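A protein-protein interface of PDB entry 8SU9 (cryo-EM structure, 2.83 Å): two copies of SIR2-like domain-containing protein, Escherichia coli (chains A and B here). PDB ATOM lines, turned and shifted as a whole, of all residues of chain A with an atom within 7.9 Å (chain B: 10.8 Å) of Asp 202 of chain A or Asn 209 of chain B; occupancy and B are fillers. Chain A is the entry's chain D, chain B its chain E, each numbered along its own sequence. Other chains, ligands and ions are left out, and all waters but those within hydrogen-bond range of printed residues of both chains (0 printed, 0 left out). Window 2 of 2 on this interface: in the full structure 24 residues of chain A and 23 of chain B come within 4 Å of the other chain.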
ATOM      1  N   PHE A 185       0.794  27.339  27.471  1.00  0.00           N
ATOM      2  CA  PHE A 185       2.243  27.486  27.444  1.00  0.00           C
ATOM      3  C   PHE A 185       2.634  28.669  28.320  1.00  0.00           C
ATOM      4  O   PHE A 185       2.098  29.770  28.153  1.00  0.00           O
ATOM      5  CB  PHE A 185       2.744  27.691  26.016  1.00  0.00           C
ATOM      6  CG  PHE A 185       2.367  26.586  25.072  1.00  0.00           C
ATOM      7  CD1 PHE A 185       2.664  25.269  25.370  1.00  0.00           C
ATOM      8  CD2 PHE A 185       1.721  26.867  23.881  1.00  0.00           C
ATOM      9  CE1 PHE A 185       2.321  24.253  24.497  1.00  0.00           C
ATOM     10  CE2 PHE A 185       1.377  25.855  23.007  1.00  0.00           C
ATOM     11  CZ  PHE A 185       1.676  24.549  23.316  1.00  0.00           C
ATOM     12  N   TYR A 197      12.761  28.163  29.613  1.00  0.00           N
ATOM     13  CA  TYR A 197      13.384  28.368  28.309  1.00  0.00           C
ATOM     14  C   TYR A 197      12.621  29.465  27.579  1.00  0.00           C
ATOM     15  O   TYR A 197      11.423  29.286  27.276  1.00  0.00           O
ATOM     16  CB  TYR A 197      13.395  27.077  27.486  1.00  0.00           C
ATOM     17  CG  TYR A 197      14.306  26.000  28.028  1.00  0.00           C
ATOM     18  CD1 TYR A 197      15.678  26.188  28.085  1.00  0.00           C
ATOM     19  CD2 TYR A 197      13.793  24.788  28.471  1.00  0.00           C
ATOM     20  CE1 TYR A 197      16.512  25.205  28.574  1.00  0.00           C
ATOM     21  CE2 TYR A 197      14.621  23.801  28.961  1.00  0.00           C
ATOM     22  CZ  TYR A 197      15.979  24.014  29.009  1.00  0.00           C
ATOM     23  OH  TYR A 197      16.807  23.032  29.498  1.00  0.00           O
ATOM     24  N   PRO A 198      13.251  30.603  27.273  1.00  0.00           N
ATOM     25  CA  PRO A 198      12.520  31.697  26.614  1.00  0.00           C
ATOM     26  C   PRO A 198      12.157  31.421  25.162  1.00  0.00           C
ATOM     27  O   PRO A 198      11.375  32.190  24.589  1.00  0.00           O
ATOM     28  CB  PRO A 198      13.490  32.880  26.723  1.00  0.00           C
ATOM     29  CG  PRO A 198      14.828  32.262  26.860  1.00  0.00           C
ATOM     30  CD  PRO A 198      14.631  30.982  27.613  1.00  0.00           C
ATOM     31  N   GLN A 199      12.686  30.366  24.550  1.00  0.00           N
ATOM     32  CA  GLN A 199      12.382  30.045  23.162  1.00  0.00           C
ATOM     33  C   GLN A 199      11.128  29.195  23.007  1.00  0.00           C
ATOM     34  O   GLN A 199      10.731  28.908  21.874  1.00  0.00           O
ATOM     35  CB  GLN A 199      13.568  29.322  22.517  1.00  0.00           C
ATOM     36  CG  GLN A 199      14.831  30.161  22.422  1.00  0.00           C
ATOM     37  CD  GLN A 199      15.762  29.946  23.600  1.00  0.00           C
ATOM     38  OE1 GLN A 199      15.875  28.838  24.122  1.00  0.00           O
ATOM     39  NE2 GLN A 199      16.435  31.010  24.023  1.00  0.00           N
ATOM     40  N   ASN A 200      10.499  28.789  24.107  1.00  0.00           N
ATOM     41  CA  ASN A 200       9.294  27.972  24.051  1.00  0.00           C
ATOM     42  C   ASN A 200       8.049  28.773  23.704  1.00  0.00           C
ATOM     43  O   ASN A 200       6.971  28.183  23.567  1.00  0.00           O
ATOM     44  CB  ASN A 200       9.084  27.250  25.383  1.00  0.00           C
ATOM     45  CG  ASN A 200       9.998  26.053  25.549  1.00  0.00           C
ATOM     46  OD1 ASN A 200      10.398  25.425  24.571  1.00  0.00           O
ATOM     47  ND2 ASN A 200      10.334  25.734  26.793  1.00  0.00           N
ATOM     48  N   PHE A 201       8.163  30.090  23.566  1.00  0.00           N
ATOM     49  CA  PHE A 201       7.033  30.944  23.232  1.00  0.00           C
ATOM     50  C   PHE A 201       6.784  31.035  21.733  1.00  0.00           C
ATOM     51  O   PHE A 201       5.883  31.767  21.315  1.00  0.00           O
ATOM     52  CB  PHE A 201       7.251  32.347  23.805  1.00  0.00           C
ATOM     53  CG  PHE A 201       6.871  32.477  25.252  1.00  0.00           C
ATOM     54  CD1 PHE A 201       5.565  32.288  25.660  1.00  0.00           C
ATOM     55  CD2 PHE A 201       7.826  32.783  26.206  1.00  0.00           C
ATOM     56  CE1 PHE A 201       5.216  32.410  26.985  1.00  0.00           C
ATOM     57  CE2 PHE A 201       7.481  32.903  27.534  1.00  0.00           C
ATOM     58  CZ  PHE A 201       6.175  32.715  27.923  1.00  0.00           C
ATOM     59  N   ASP A 202       7.557  30.317  20.917  1.00  0.00           N
ATOM     60  CA  ASP A 202       7.406  30.335  19.467  1.00  0.00           C
ATOM     61  C   ASP A 202       7.064  28.954  18.914  1.00  0.00           C
ATOM     62  O   ASP A 202       7.573  28.558  17.866  1.00  0.00           O
ATOM     63  CB  ASP A 202       8.671  30.872  18.799  1.00  0.00           C
ATOM     64  CG  ASP A 202       8.971  32.305  19.180  1.00  0.00           C
ATOM     65  OD1 ASP A 202       8.111  33.178  18.941  1.00  0.00           O
ATOM     66  OD2 ASP A 202      10.072  32.564  19.710  1.00  0.00           O
ATOM     67  N   LEU A 203       6.204  28.210  19.605  1.00  0.00           N
ATOM     68  CA  LEU A 203       5.827  26.868  19.188  1.00  0.00           C
ATOM     69  C   LEU A 203       4.310  26.737  19.161  1.00  0.00           C
ATOM     70  O   LEU A 203       3.588  27.471  19.840  1.00  0.00           O
ATOM     71  CB  LEU A 203       6.424  25.800  20.113  1.00  0.00           C
ATOM     72  CG  LEU A 203       7.948  25.686  20.131  1.00  0.00           C
ATOM     73  CD1 LEU A 203       8.396  24.700  21.194  1.00  0.00           C
ATOM     74  CD2 LEU A 203       8.470  25.277  18.765  1.00  0.00           C
ATOM     75  N   ALA A 204       3.835  25.786  18.360  1.00  0.00           N
ATOM     76  CA  ALA A 204       2.411  25.520  18.231  1.00  0.00           C
ATOM     77  C   ALA A 204       2.212  24.038  17.943  1.00  0.00           C
ATOM     78  O   ALA A 204       3.169  23.296  17.714  1.00  0.00           O
ATOM     79  CB  ALA A 204       1.779  26.381  17.133  1.00  0.00           C
ATOM     80  N   TYR A 222      -1.665  31.192  25.322  1.00  0.00           N
ATOM     81  CA  TYR A 222      -0.413  31.609  25.934  1.00  0.00           C
ATOM     82  C   TYR A 222      -0.700  32.380  27.214  1.00  0.00           C
ATOM     83  O   TYR A 222      -1.611  33.211  27.256  1.00  0.00           O
ATOM     84  CB  TYR A 222       0.415  32.470  24.973  1.00  0.00           C
ATOM     85  CG  TYR A 222       0.903  31.712  23.762  1.00  0.00           C
ATOM     86  CD1 TYR A 222       1.979  30.843  23.850  1.00  0.00           C
ATOM     87  CD2 TYR A 222       0.282  31.859  22.531  1.00  0.00           C
ATOM     88  CE1 TYR A 222       2.424  30.143  22.749  1.00  0.00           C
ATOM     89  CE2 TYR A 222       0.720  31.163  21.424  1.00  0.00           C
ATOM     90  CZ  TYR A 222       1.791  30.307  21.538  1.00  0.00           C
ATOM     91  OH  TYR A 222       2.232  29.613  20.439  1.00  0.00           O
ATOM     92  N   TYR A 224       1.070  34.657  30.420  1.00  0.00           N
ATOM     93  CA  TYR A 224       2.199  35.454  30.887  1.00  0.00           C
ATOM     94  C   TYR A 224       1.911  35.926  32.303  1.00  0.00           C
ATOM     95  O   TYR A 224       0.875  36.554  32.551  1.00  0.00           O
ATOM     96  CB  TYR A 224       2.450  36.651  29.967  1.00  0.00           C
ATOM     97  CG  TYR A 224       2.583  36.307  28.501  1.00  0.00           C
ATOM     98  CD1 TYR A 224       1.465  36.209  27.687  1.00  0.00           C
ATOM     99  CD2 TYR A 224       3.827  36.095  27.929  1.00  0.00           C
ATOM    100  CE1 TYR A 224       1.583  35.901  26.349  1.00  0.00           C
ATOM    101  CE2 TYR A 224       3.952  35.786  26.592  1.00  0.00           C
ATOM    102  CZ  TYR A 224       2.827  35.692  25.807  1.00  0.00           C
ATOM    103  OH  TYR A 224       2.946  35.383  24.475  1.00  0.00           O
ATOM    104  N   GLU A 286      11.983  39.467  30.336  1.00  0.00           N
ATOM    105  CA  GLU A 286      11.421  38.652  29.268  1.00  0.00           C
ATOM    106  C   GLU A 286       9.906  38.759  29.197  1.00  0.00           C
ATOM    107  O   GLU A 286       9.346  38.793  28.095  1.00  0.00           O
ATOM    108  CB  GLU A 286      11.826  37.188  29.448  1.00  0.00           C
ATOM    109  CG  GLU A 286      11.443  36.295  28.284  1.00  0.00           C
ATOM    110  CD  GLU A 286      12.301  36.541  27.062  1.00  0.00           C
ATOM    111  OE1 GLU A 286      13.491  36.879  27.229  1.00  0.00           O
ATOM    112  OE2 GLU A 286      11.787  36.399  25.933  1.00  0.00           O
ATOM    113  N   ARG A 289       9.111  42.242  27.804  1.00  0.00           N
ATOM    114  CA  ARG A 289       9.508  42.452  26.421  1.00  0.00           C
ATOM    115  C   ARG A 289       8.499  41.879  25.437  1.00  0.00           C
ATOM    116  O   ARG A 289       8.519  42.252  24.260  1.00  0.00           O
ATOM    117  CB  ARG A 289      10.887  41.839  26.171  1.00  0.00           C
ATOM    118  CG  ARG A 289      11.664  42.495  25.042  1.00  0.00           C
ATOM    119  CD  ARG A 289      11.792  41.577  23.843  1.00  0.00           C
ATOM    120  NE  ARG A 289      12.561  40.379  24.154  1.00  0.00           N
ATOM    121  CZ  ARG A 289      12.548  39.272  23.424  1.00  0.00           C
ATOM    122  NH1 ARG A 289      11.815  39.175  22.328  1.00  0.00           N
ATOM    123  NH2 ARG A 289      13.288  38.235  23.805  1.00  0.00           N
ATOM    124  N   ARG A 290       7.615  40.993  25.894  1.00  0.00           N
ATOM    125  CA  ARG A 290       6.586  40.420  25.036  1.00  0.00           C
ATOM    126  C   ARG A 290       5.264  41.168  25.127  1.00  0.00           C
ATOM    127  O   ARG A 290       4.442  41.068  24.210  1.00  0.00           O
ATOM    128  CB  ARG A 290       6.372  38.947  25.389  1.00  0.00           C
ATOM    129  CG  ARG A 290       7.635  38.108  25.306  1.00  0.00           C
ATOM    130  CD  ARG A 290       7.580  37.139  24.143  1.00  0.00           C
ATOM    131  NE  ARG A 290       8.803  36.356  24.024  1.00  0.00           N
ATOM    132  CZ  ARG A 290       9.071  35.542  23.013  1.00  0.00           C
ATOM    133  NH1 ARG A 290       8.221  35.375  22.015  1.00  0.00           N
ATOM    134  NH2 ARG A 290      10.225  34.879  23.004  1.00  0.00           N
ATOM    135  N   GLU A 293       5.749  44.117  22.637  1.00  0.00           N
ATOM    136  CA  GLU A 293       5.737  43.625  21.266  1.00  0.00           C
ATOM    137  C   GLU A 293       4.334  43.247  20.807  1.00  0.00           C
ATOM    138  O   GLU A 293       4.043  43.304  19.607  1.00  0.00           O
ATOM    139  CB  GLU A 293       6.678  42.426  21.142  1.00  0.00           C
ATOM    140  CG  GLU A 293       6.830  41.878  19.734  1.00  0.00           C
ATOM    141  CD  GLU A 293       7.906  40.816  19.638  1.00  0.00           C
ATOM    142  OE1 GLU A 293       8.527  40.503  20.675  1.00  0.00           O
ATOM    143  OE2 GLU A 293       8.132  40.295  18.526  1.00  0.00           O
ATOM    144  N   GLN B 183      12.095  17.005  24.148  1.00  0.00           N
ATOM    145  CA  GLN B 183      10.807  16.710  24.763  1.00  0.00           C
ATOM    146  C   GLN B 183      10.282  15.389  24.222  1.00  0.00           C
ATOM    147  O   GLN B 183      10.260  15.178  23.007  1.00  0.00           O
ATOM    148  CB  GLN B 183       9.803  17.832  24.497  1.00  0.00           C
ATOM    149  CG  GLN B 183      10.321  19.215  24.846  1.00  0.00           C
ATOM    150  CD  GLN B 183       9.230  20.263  24.843  1.00  0.00           C
ATOM    151  OE1 GLN B 183       8.042  19.940  24.814  1.00  0.00           O
ATOM    152  NE2 GLN B 183       9.627  21.529  24.877  1.00  0.00           N
ATOM    153  N   ALA B 204       2.408  17.070  16.886  1.00  0.00           N
ATOM    154  CA  ALA B 204       3.770  17.473  16.576  1.00  0.00           C
ATOM    155  C   ALA B 204       3.896  18.977  16.760  1.00  0.00           C
ATOM    156  O   ALA B 204       2.899  19.698  16.830  1.00  0.00           O
ATOM    157  CB  ALA B 204       4.167  17.071  15.150  1.00  0.00           C
ATOM    158  N   PHE B 205       5.137  19.440  16.843  1.00  0.00           N
ATOM    159  CA  PHE B 205       5.441  20.850  17.028  1.00  0.00           C
ATOM    160  C   PHE B 205       5.758  21.515  15.694  1.00  0.00           C
ATOM    161  O   PHE B 205       6.095  20.857  14.705  1.00  0.00           O
ATOM    162  CB  PHE B 205       6.619  21.031  17.989  1.00  0.00           C
ATOM    163  CG  PHE B 205       6.239  20.956  19.439  1.00  0.00           C
ATOM    164  CD1 PHE B 205       5.140  21.645  19.918  1.00  0.00           C
ATOM    165  CD2 PHE B 205       6.985  20.202  20.325  1.00  0.00           C
ATOM    166  CE1 PHE B 205       4.791  21.578  21.252  1.00  0.00           C
ATOM    167  CE2 PHE B 205       6.641  20.131  21.659  1.00  0.00           C
ATOM    168  CZ  PHE B 205       5.544  20.819  22.122  1.00  0.00           C
ATOM    169  N   ARG B 206       5.643  22.840  15.679  1.00  0.00           N
ATOM    170  CA  ARG B 206       6.019  23.634  14.518  1.00  0.00           C
ATOM    171  C   ARG B 206       6.371  25.037  14.986  1.00  0.00           C
ATOM    172  O   ARG B 206       6.025  25.444  16.097  1.00  0.00           O
ATOM    173  CB  ARG B 206       4.906  23.673  13.467  1.00  0.00           C
ATOM    174  CG  ARG B 206       3.730  24.555  13.833  1.00  0.00           C
ATOM    175  CD  ARG B 206       2.627  24.447  12.795  1.00  0.00           C
ATOM    176  NE  ARG B 206       1.384  25.057  13.250  1.00  0.00           N
ATOM    177  CZ  ARG B 206       1.099  26.347  13.135  1.00  0.00           C
ATOM    178  NH1 ARG B 206       1.947  27.196  12.577  1.00  0.00           N
ATOM    179  NH2 ARG B 206      -0.067  26.797  13.591  1.00  0.00           N
ATOM    180  N   ASN B 207       7.063  25.769  14.122  1.00  0.00           N
ATOM    181  CA  ASN B 207       7.517  27.118  14.421  1.00  0.00           C
ATOM    182  C   ASN B 207       6.593  28.137  13.768  1.00  0.00           C
ATOM    183  O   ASN B 207       6.187  27.972  12.614  1.00  0.00           O
ATOM    184  CB  ASN B 207       8.952  27.326  13.936  1.00  0.00           C
ATOM    185  CG  ASN B 207       9.706  28.340  14.767  1.00  0.00           C
ATOM    186  OD1 ASN B 207       9.127  29.304  15.267  1.00  0.00           O
ATOM    187  ND2 ASN B 207      11.006  28.127  14.924  1.00  0.00           N
ATOM    188  N   VAL B 208       6.263  29.192  14.517  1.00  0.00           N
ATOM    189  CA  VAL B 208       5.338  30.209  14.019  1.00  0.00           C
ATOM    190  C   VAL B 208       6.015  31.272  13.170  1.00  0.00           C
ATOM    191  O   VAL B 208       5.323  32.139  12.621  1.00  0.00           O
ATOM    192  CB  VAL B 208       4.599  30.896  15.180  1.00  0.00           C
ATOM    193  CG1 VAL B 208       3.722  29.897  15.912  1.00  0.00           C
ATOM    194  CG2 VAL B 208       5.593  31.537  16.131  1.00  0.00           C
ATOM    195  N   ASN B 209       7.340  31.237  13.046  1.00  0.00           N
ATOM    196  CA  ASN B 209       8.077  32.205  12.245  1.00  0.00           C
ATOM    197  C   ASN B 209       8.599  31.620  10.943  1.00  0.00           C
ATOM    198  O   ASN B 209       8.375  32.195   9.872  1.00  0.00           O
ATOM    199  CB  ASN B 209       9.245  32.782  13.057  1.00  0.00           C
ATOM    200  CG  ASN B 209       8.852  33.125  14.476  1.00  0.00           C
ATOM    201  OD1 ASN B 209       7.867  33.825  14.707  1.00  0.00           O
ATOM    202  ND2 ASN B 209       9.625  32.636  15.438  1.00  0.00           N
ATOM    203  N   ALA B 210       9.293  30.488  11.002  1.00  0.00           N
ATOM    204  CA  ALA B 210       9.836  29.860   9.804  1.00  0.00           C
ATOM    205  C   ALA B 210       8.725  29.254   8.954  1.00  0.00           C
ATOM    206  O   ALA B 210       7.699  28.819   9.475  1.00  0.00           O
ATOM    207  CB  ALA B 210      10.858  28.798  10.179  1.00  0.00           C
ATOM    208  N   GLY B 217      12.373  23.282  17.846  1.00  0.00           N
ATOM    209  CA  GLY B 217      11.700  23.049  16.584  1.00  0.00           C
ATOM    210  C   GLY B 217      11.316  21.598  16.387  1.00  0.00           C
ATOM    211  O   GLY B 217      10.457  21.072  17.094  1.00  0.00           O
ATOM    212  N   HIS B 218      11.961  20.944  15.420  1.00  0.00           N
ATOM    213  CA  HIS B 218      11.711  19.532  15.129  1.00  0.00           C
ATOM    214  C   HIS B 218      12.545  18.639  16.050  1.00  0.00           C
ATOM    215  O   HIS B 218      13.295  17.765  15.618  1.00  0.00           O
ATOM    216  CB  HIS B 218      12.000  19.236  13.663  1.00  0.00           C
ATOM    217  CG  HIS B 218      11.046  19.891  12.713  1.00  0.00           C
ATOM    218  ND1 HIS B 218      11.465  20.690  11.672  1.00  0.00           N
ATOM    219  CD2 HIS B 218       9.695  19.861  12.644  1.00  0.00           C
ATOM    220  CE1 HIS B 218      10.412  21.127  11.003  1.00  0.00           C
ATOM    221  NE2 HIS B 218       9.325  20.639  11.573  1.00  0.00           N
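The backbone NH (N) of Ala 204 of chain A sits at hydrogen-bond distance from the backbone carbonyl oxygen (O) of Arg 206 of chain B, at 3.2 Å.
The side-chain amide oxygen (OD1) of Asn 207 of chain B sits close to the backbone carbonyl oxygen (O) of Asp 202 of chain A (3.1 Å).
O of Leu 203 of chain A sits at hydrogen-bond distance from OH of Tyr 222 of chain A.
NH1 of Arg 290 of chain A is in salt-bridge range of OD1 of Asp 202 of chain A (3.8 Å).
The side-chain amide oxygen (OD1) of Asn 207 of chain B lies within hydrogen-bond range of the side-chain amide nitrogen (ND2) of Asn 209 of chain B.
Among the printed residues, merely in contact across the chains: Asn 200 of chain A with Gln 183 of chain B (3.98 Å), Asp 202 of chain A with Arg 206 of chain B (3.9 Å), Asp 202 of chain A with Val 208 of chain B (3.7 Å), Asp 202 of chain A with Asn 209 of chain B (3.8 Å), Leu 203 of chain A with Arg 206 of chain B (3.4 Å), Ala 204 of chain A with Ala 204 of chain B (3.7 Å) and Ala 204 of chain A with Phe 205 of chain B (3.4 Å).
Asp 202 of chain A touches just these residues of chain B: Arg 206 (3.9 Å), Asn 207 (3.1 Å), Val 208 (3.7 Å) and Asn 209 (3.8 Å).
Asn 209 of chain B touches one residue of chain A.
Leu 203 of chain A touches just one residue of chain B: Arg 206.
Ala 210 of chain B touches none of the printed residues of chain A.
Printed residues of chain A within 4 Å of Asn 207 of chain B: Asp 202.
Printed residues of chain A within 4 Å of Val 208 of chain B: Asp 202 (3.7 Å).
Of the printed residues of chain A, Phe 205 of chain B touches Ala 204 (3.4 Å).
Of the printed residues of chain A, Arg 206 of chain B touches Asp 202, Leu 203 and Ala 204.
Gln 199 of chain A touches none of the printed residues of chain B.
Tyr 197 of chain A touches none of the printed residues of chain B.
The nearest residue of chain A that does not touch Asn 209 of chain B is Leu 203 of chain A (7.0 Å).
Of the 15 printed residues of chain A, 4 touch a printed residue of chain B.
Among the printed residues, no Asp or Glu carboxylate lies within 4 Å of a Lys or Arg side-chain nitrogen of the other chain.
Ala 204 of chain B touches its own counterpart, Ala 204 of chain A.
Of the 9 pairs that touch across the chains among the printed residues, 1 has its exchanged pair printed and touching as well.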
